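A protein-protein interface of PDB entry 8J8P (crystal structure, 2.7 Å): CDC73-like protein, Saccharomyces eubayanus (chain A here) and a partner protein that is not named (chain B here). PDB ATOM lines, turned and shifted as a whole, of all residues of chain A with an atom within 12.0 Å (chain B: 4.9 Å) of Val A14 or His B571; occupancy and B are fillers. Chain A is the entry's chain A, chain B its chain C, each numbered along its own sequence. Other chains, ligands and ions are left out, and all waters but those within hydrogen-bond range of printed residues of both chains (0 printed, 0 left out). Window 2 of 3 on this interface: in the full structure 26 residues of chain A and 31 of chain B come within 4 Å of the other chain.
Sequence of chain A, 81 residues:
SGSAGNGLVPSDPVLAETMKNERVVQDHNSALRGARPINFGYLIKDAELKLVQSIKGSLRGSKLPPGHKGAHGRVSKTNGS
His B571 touches Val A14 (CD2 to CG1, 3.8 Å).
Glu A17 touches Ser B539.
CD1 of Ile B542 touches OG1 of Thr A18, 3.9 Å away.
Of the 11 printed residues of chain B, 4 touch a printed residue of chain A.
Printed residues of chain B that touch a printed residue of chain A: Ser B539, Ile B542, His B571 and Tyr B574.
Hydrophobic or aromatic side chains of chain B within 4 Å of the printed part of chain A: Ile B542, His B571 and Tyr B574.
Along chain B the printed residues that touch a printed residue of chain A span positions 539 to 574.
Of the 12 printed residues of chain A, 4 touch a printed residue of chain B.
Printed residues of chain A that touch a printed residue of chain B: Val A14, Glu A17, Thr A18 and Glu A22.
Hydrophobic or aromatic side chains of chain A that line the printed part of chain B: Val A14.
Among the printed residues, no Asp or Glu carboxylate lies within 4 Å of a Lys or Arg side-chain nitrogen of the other chain.
The side-chain hydroxyl of Tyr B574 is in hydrogen-bond range of the side-chain carboxylate of Glu A22 (3.2 Å).
The backbone carbonyl oxygen (O) of Ser B539 lies within hydrogen-bond range of the side-chain hydroxyl (OG1) of Thr A18 (2.6 Å).
OG of Ser B539 sits at hydrogen-bond distance from O of Asn B537, 3.3 Å away.
The side-chain amide nitrogen (ND2) of Asn A21 lies within hydrogen-bond range of the side-chain carboxylate (OE1) of Glu A17, at 3.2 Å.
Val A14 touches one residue of chain B.
Printed residues of chain B within 4 Å of Glu A17: Ser B539.
Printed residues of chain B within 4 Å of Thr A18: Ser B539 (2.6 Å) and Ile B542 (3.9 Å).
Met A19 touches none of the printed residues of chain B.
Asn B537 touches none of the printed residues of chain A.
Of chain A, only Glu A17 and Thr A18 come within 4 Å of Ser B539.
No residue of chain A comes within 4 Å of Ile B567.
No residue of chain A comes within 4 Å of Ser B570.
His B571 touches just one residue of chain A: Val A14 (3.8 Å).
No residue of chain A comes within 4 Å of Pro B572.
No residue of chain A comes within 4 Å of Ser B573.
Of the printed residues of chain A, Tyr B574 touches Glu A22 (3.2 Å).
The nearest printed residue of chain A that does not touch His B571 is Leu A15 (4.03 Å).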
ATOM      1  N   SER A  11     -29.883 -21.284  14.903  1.00  0.00           N
ATOM      2  CA  SER A  11     -30.751 -21.962  13.947  1.00  0.00           C
ATOM      3  C   SER A  11     -29.928 -22.587  12.826  1.00  0.00           C
ATOM      4  O   SER A  11     -29.135 -23.500  13.068  1.00  0.00           O
ATOM      5  CB  SER A  11     -31.787 -20.992  13.371  1.00  0.00           C
ATOM      6  OG  SER A  11     -32.747 -21.676  12.581  1.00  0.00           O
ATOM      7  N   ASP A  12     -30.117 -22.088  11.603  1.00  0.00           N
ATOM      8  CA  ASP A  12     -29.398 -22.634  10.454  1.00  0.00           C
ATOM      9  C   ASP A  12     -27.903 -22.362  10.598  1.00  0.00           C
ATOM     10  O   ASP A  12     -27.505 -21.216  10.846  1.00  0.00           O
ATOM     11  CB  ASP A  12     -29.928 -22.045   9.142  1.00  0.00           C
ATOM     12  CG  ASP A  12     -29.772 -20.535   9.064  1.00  0.00           C
ATOM     13  OD1 ASP A  12     -30.406 -19.827   9.876  1.00  0.00           O
ATOM     14  OD2 ASP A  12     -29.020 -20.056   8.184  1.00  0.00           O
ATOM     15  N   PRO A  13     -27.049 -23.379  10.465  1.00  0.00           N
ATOM     16  CA  PRO A  13     -25.615 -23.186  10.694  1.00  0.00           C
ATOM     17  C   PRO A  13     -24.808 -22.843   9.454  1.00  0.00           C
ATOM     18  O   PRO A  13     -23.618 -22.520   9.587  1.00  0.00           O
ATOM     19  CB  PRO A  13     -25.180 -24.544  11.272  1.00  0.00           C
ATOM     20  CG  PRO A  13     -26.247 -25.536  10.829  1.00  0.00           C
ATOM     21  CD  PRO A  13     -27.371 -24.783  10.168  1.00  0.00           C
ATOM     22  N   VAL A  14     -25.399 -22.908   8.260  1.00  0.00           N
ATOM     23  CA  VAL A  14     -24.694 -22.434   7.074  1.00  0.00           C
ATOM     24  C   VAL A  14     -24.383 -20.948   7.216  1.00  0.00           C
ATOM     25  O   VAL A  14     -23.298 -20.482   6.842  1.00  0.00           O
ATOM     26  CB  VAL A  14     -25.513 -22.742   5.805  1.00  0.00           C
ATOM     27  CG1 VAL A  14     -26.978 -22.346   5.994  1.00  0.00           C
ATOM     28  CG2 VAL A  14     -24.903 -22.061   4.587  1.00  0.00           C
ATOM     29  N   LEU A  15     -25.323 -20.187   7.786  1.00  0.00           N
ATOM     30  CA  LEU A  15     -25.037 -18.823   8.204  1.00  0.00           C
ATOM     31  C   LEU A  15     -24.055 -18.792   9.370  1.00  0.00           C
ATOM     32  O   LEU A  15     -23.320 -17.811   9.523  1.00  0.00           O
ATOM     33  CB  LEU A  15     -26.346 -18.114   8.580  1.00  0.00           C
ATOM     34  CG  LEU A  15     -26.489 -16.584   8.584  1.00  0.00           C
ATOM     35  CD1 LEU A  15     -25.646 -15.919   9.670  1.00  0.00           C
ATOM     36  CD2 LEU A  15     -26.174 -15.996   7.211  1.00  0.00           C
ATOM     37  N   ALA A  16     -23.927 -19.847  10.131  1.00  0.00           N
ATOM     38  CA  ALA A  16     -22.972 -19.802  11.233  1.00  0.00           C
ATOM     39  C   ALA A  16     -21.479 -19.623  10.884  1.00  0.00           C
ATOM     40  O   ALA A  16     -20.741 -18.824  11.502  1.00  0.00           O
ATOM     41  CB  ALA A  16     -23.157 -21.010  12.104  1.00  0.00           C
ATOM     42  N   GLU A  17     -21.005 -20.281   9.831  1.00  0.00           N
ATOM     43  CA  GLU A  17     -19.575 -20.153   9.460  1.00  0.00           C
ATOM     44  C   GLU A  17     -19.237 -18.723   9.106  1.00  0.00           C
ATOM     45  O   GLU A  17     -18.216 -18.196   9.517  1.00  0.00           O
ATOM     46  CB  GLU A  17     -19.190 -21.083   8.321  1.00  0.00           C
ATOM     47  CG  GLU A  17     -18.286 -22.221   8.749  1.00  0.00           C
ATOM     48  CD  GLU A  17     -17.522 -21.938  10.031  1.00  0.00           C
ATOM     49  OE1 GLU A  17     -16.444 -21.322   9.942  1.00  0.00           O
ATOM     50  OE2 GLU A  17     -17.976 -22.346  11.122  1.00  0.00           O
ATOM     51  N   THR A  18     -20.167 -18.119   8.372  1.00  0.00           N
ATOM     52  CA  THR A  18     -20.091 -16.727   7.987  1.00  0.00           C
ATOM     53  C   THR A  18     -20.160 -15.892   9.259  1.00  0.00           C
ATOM     54  O   THR A  18     -19.439 -14.903   9.385  1.00  0.00           O
ATOM     55  CB  THR A  18     -21.249 -16.331   7.054  1.00  0.00           C
ATOM     56  OG1 THR A  18     -20.904 -16.651   5.699  1.00  0.00           O
ATOM     57  CG2 THR A  18     -21.533 -14.840   7.161  1.00  0.00           C
ATOM     58  N   MET A  19     -21.020 -16.277  10.206  1.00  0.00           N
ATOM     59  CA  MET A  19     -21.077 -15.510  11.410  1.00  0.00           C
ATOM     60  C   MET A  19     -19.697 -15.393  12.038  1.00  0.00           C
ATOM     61  O   MET A  19     -19.322 -14.298  12.390  1.00  0.00           O
ATOM     62  CB  MET A  19     -22.136 -16.089  12.406  1.00  0.00           C
ATOM     63  CG  MET A  19     -21.652 -16.721  13.736  1.00  0.00           C
ATOM     64  SD  MET A  19     -22.884 -17.337  14.931  1.00  0.00           S
ATOM     65  CE  MET A  19     -21.887 -18.152  16.153  1.00  0.00           C
ATOM     66  N   LYS A  20     -18.885 -16.438  12.079  1.00  0.00           N
ATOM     67  CA  LYS A  20     -17.603 -16.247  12.771  1.00  0.00           C
ATOM     68  C   LYS A  20     -16.324 -15.885  12.031  1.00  0.00           C
ATOM     69  O   LYS A  20     -15.297 -15.695  12.618  1.00  0.00           O
ATOM     70  CB  LYS A  20     -17.347 -17.417  13.696  1.00  0.00           C
ATOM     71  CG  LYS A  20     -18.073 -17.300  15.013  1.00  0.00           C
ATOM     72  CD  LYS A  20     -17.217 -16.717  16.118  1.00  0.00           C
ATOM     73  CE  LYS A  20     -18.070 -16.416  17.340  1.00  0.00           C
ATOM     74  NZ  LYS A  20     -19.222 -15.508  17.077  1.00  0.00           N
ATOM     75  N   ASN A  21     -16.412 -15.848  10.699  1.00  0.00           N
ATOM     76  CA  ASN A  21     -15.261 -15.527   9.845  1.00  0.00           C
ATOM     77  C   ASN A  21     -15.175 -14.106   9.256  1.00  0.00           C
ATOM     78  O   ASN A  21     -14.143 -13.734   8.697  1.00  0.00           O
ATOM     79  CB  ASN A  21     -15.149 -16.556   8.713  1.00  0.00           C
ATOM     80  CG  ASN A  21     -14.492 -17.847   9.162  1.00  0.00           C
ATOM     81  OD1 ASN A  21     -13.500 -18.287   8.581  1.00  0.00           O
ATOM     82  ND2 ASN A  21     -15.046 -18.460  10.202  1.00  0.00           N
ATOM     83  N   GLU A  22     -16.239 -13.316   9.376  1.00  0.00           N
ATOM     84  CA  GLU A  22     -16.241 -11.957   8.853  1.00  0.00           C
ATOM     85  C   GLU A  22     -16.069 -10.969   9.999  1.00  0.00           C
ATOM     86  O   GLU A  22     -16.679 -11.127  11.061  1.00  0.00           O
ATOM     87  CB  GLU A  22     -17.532 -11.648   8.084  1.00  0.00           C
ATOM     88  CG  GLU A  22     -18.805 -12.049   8.807  1.00  0.00           C
ATOM     89  CD  GLU A  22     -20.029 -11.312   8.290  1.00  0.00           C
ATOM     90  OE1 GLU A  22     -20.065 -10.976   7.088  1.00  0.00           O
ATOM     91  OE2 GLU A  22     -20.963 -11.071   9.087  1.00  0.00           O
ATOM     92  N   ASN B 537     -18.902 -26.110   2.460  1.00  0.00           N
ATOM     93  CA  ASN B 537     -19.596 -25.032   3.166  1.00  0.00           C
ATOM     94  C   ASN B 537     -19.012 -23.675   2.769  1.00  0.00           C
ATOM     95  O   ASN B 537     -18.429 -22.944   3.572  1.00  0.00           O
ATOM     96  CB  ASN B 537     -19.550 -25.230   4.687  1.00  0.00           C
ATOM     97  CG  ASN B 537     -20.565 -24.359   5.428  1.00  0.00           C
ATOM     98  OD1 ASN B 537     -21.003 -23.320   4.929  1.00  0.00           O
ATOM     99  ND2 ASN B 537     -20.945 -24.789   6.628  1.00  0.00           N
ATOM    100  N   SER B 539     -19.291 -20.733   2.882  1.00  0.00           N
ATOM    101  CA  SER B 539     -19.891 -19.591   3.558  1.00  0.00           C
ATOM    102  C   SER B 539     -19.305 -18.274   3.078  1.00  0.00           C
ATOM    103  O   SER B 539     -19.837 -17.215   3.422  1.00  0.00           O
ATOM    104  CB  SER B 539     -19.713 -19.720   5.073  1.00  0.00           C
ATOM    105  OG  SER B 539     -18.431 -20.229   5.402  1.00  0.00           O
ATOM    106  N   ILE B 542     -21.774 -15.828   0.703  1.00  0.00           N
ATOM    107  CA  ILE B 542     -22.704 -14.872   1.298  1.00  0.00           C
ATOM    108  C   ILE B 542     -22.015 -13.521   1.490  1.00  0.00           C
ATOM    109  O   ILE B 542     -22.513 -12.472   1.053  1.00  0.00           O
ATOM    110  CB  ILE B 542     -23.268 -15.431   2.616  1.00  0.00           C
ATOM    111  CG1 ILE B 542     -23.914 -16.798   2.379  1.00  0.00           C
ATOM    112  CG2 ILE B 542     -24.296 -14.495   3.193  1.00  0.00           C
ATOM    113  CD1 ILE B 542     -23.025 -17.981   2.719  1.00  0.00           C
ATOM    114  N   ILE B 567     -29.965 -13.167  -1.510  1.00  0.00           N
ATOM    115  CA  ILE B 567     -29.300 -13.439  -0.237  1.00  0.00           C
ATOM    116  C   ILE B 567     -30.321 -13.507   0.891  1.00  0.00           C
ATOM    117  O   ILE B 567     -30.301 -14.431   1.714  1.00  0.00           O
ATOM    118  CB  ILE B 567     -28.219 -12.380   0.046  1.00  0.00           C
ATOM    119  CG1 ILE B 567     -26.979 -12.636  -0.810  1.00  0.00           C
ATOM    120  CG2 ILE B 567     -27.845 -12.371   1.524  1.00  0.00           C
ATOM    121  CD1 ILE B 567     -25.840 -11.692  -0.509  1.00  0.00           C
ATOM    122  N   THR B 568     -31.235 -12.532   0.949  1.00  0.00           N
ATOM    123  CA  THR B 568     -32.196 -12.530   2.049  1.00  0.00           C
ATOM    124  C   THR B 568     -33.232 -13.636   1.894  1.00  0.00           C
ATOM    125  O   THR B 568     -33.761 -14.128   2.898  1.00  0.00           O
ATOM    126  CB  THR B 568     -32.885 -11.169   2.178  1.00  0.00           C
ATOM    127  OG1 THR B 568     -33.841 -11.226   3.245  1.00  0.00           O
ATOM    128  CG2 THR B 568     -33.604 -10.795   0.897  1.00  0.00           C
ATOM    129  N   SER B 569     -33.526 -14.054   0.657  1.00  0.00           N
ATOM    130  CA  SER B 569     -34.435 -15.181   0.470  1.00  0.00           C
ATOM    131  C   SER B 569     -33.781 -16.489   0.898  1.00  0.00           C
ATOM    132  O   SER B 569     -34.455 -17.383   1.423  1.00  0.00           O
ATOM    133  CB  SER B 569     -34.890 -15.264  -0.988  1.00  0.00           C
ATOM    134  OG  SER B 569     -34.121 -16.209  -1.713  1.00  0.00           O
ATOM    135  N   SER B 570     -32.468 -16.619   0.690  1.00  0.00           N
ATOM    136  CA  SER B 570     -31.792 -17.864   1.040  1.00  0.00           C
ATOM    137  C   SER B 570     -31.542 -17.982   2.543  1.00  0.00           C
ATOM    138  O   SER B 570     -31.705 -19.065   3.114  1.00  0.00           O
ATOM    139  CB  SER B 570     -30.477 -17.982   0.269  1.00  0.00           C
ATOM    140  OG  SER B 570     -30.705 -17.946  -1.131  1.00  0.00           O
ATOM    141  N   HIS B 571     -31.144 -16.888   3.200  1.00  0.00           N
ATOM    142  CA  HIS B 571     -30.829 -16.921   4.627  1.00  0.00           C
ATOM    143  C   HIS B 571     -31.486 -15.725   5.308  1.00  0.00           C
ATOM    144  O   HIS B 571     -31.380 -14.592   4.805  1.00  0.00           O
ATOM    145  CB  HIS B 571     -29.314 -16.919   4.862  1.00  0.00           C
ATOM    146  CG  HIS B 571     -28.577 -17.935   4.043  1.00  0.00           C
ATOM    147  ND1 HIS B 571     -28.162 -17.690   2.750  1.00  0.00           N
ATOM    148  CD2 HIS B 571     -28.184 -19.198   4.329  1.00  0.00           C
ATOM    149  CE1 HIS B 571     -27.544 -18.758   2.277  1.00  0.00           C
ATOM    150  NE2 HIS B 571     -27.544 -19.688   3.216  1.00  0.00           N
ATOM    151  N   PRO B 572     -32.161 -15.932   6.441  1.00  0.00           N
ATOM    152  CA  PRO B 572     -33.020 -14.876   6.989  1.00  0.00           C
ATOM    153  C   PRO B 572     -32.331 -13.940   7.968  1.00  0.00           C
ATOM    154  O   PRO B 572     -32.680 -12.758   8.037  1.00  0.00           O
ATOM    155  CB  PRO B 572     -34.129 -15.675   7.682  1.00  0.00           C
ATOM    156  CG  PRO B 572     -33.424 -16.913   8.166  1.00  0.00           C
ATOM    157  CD  PRO B 572     -32.284 -17.191   7.198  1.00  0.00           C
ATOM    158  N   SER B 573     -31.358 -14.444   8.732  1.00  0.00           N
ATOM    159  CA  SER B 573     -30.790 -13.666   9.829  1.00  0.00           C
ATOM    160  C   SER B 573     -29.833 -12.573   9.365  1.00  0.00           C
ATOM    161  O   SER B 573     -29.441 -11.736  10.187  1.00  0.00           O
ATOM    162  CB  SER B 573     -30.070 -14.591  10.814  1.00  0.00           C
ATOM    163  OG  SER B 573     -29.589 -13.868  11.939  1.00  0.00           O
ATOM    164  N   TYR B 574     -29.449 -12.552   8.086  1.00  0.00           N
ATOM    165  CA  TYR B 574     -28.522 -11.532   7.609  1.00  0.00           C
ATOM    166  C   TYR B 574     -29.174 -10.156   7.610  1.00  0.00           C
ATOM    167  O   TYR B 574     -29.821  -9.759   6.633  1.00  0.00           O
ATOM    168  CB  TYR B 574     -28.005 -11.864   6.209  1.00  0.00           C
ATOM    169  CG  TYR B 574     -26.580 -11.406   5.982  1.00  0.00           C
ATOM    170  CD1 TYR B 574     -25.839 -11.882   4.913  1.00  0.00           C
ATOM    171  CD2 TYR B 574     -25.972 -10.501   6.848  1.00  0.00           C
ATOM    172  CE1 TYR B 574     -24.533 -11.466   4.705  1.00  0.00           C
ATOM    173  CE2 TYR B 574     -24.667 -10.079   6.648  1.00  0.00           C
ATOM    174  CZ  TYR B 574     -23.954 -10.568   5.573  1.00  0.00           C
ATOM    175  OH  TYR B 574     -22.658 -10.162   5.360  1.00  0.00           O
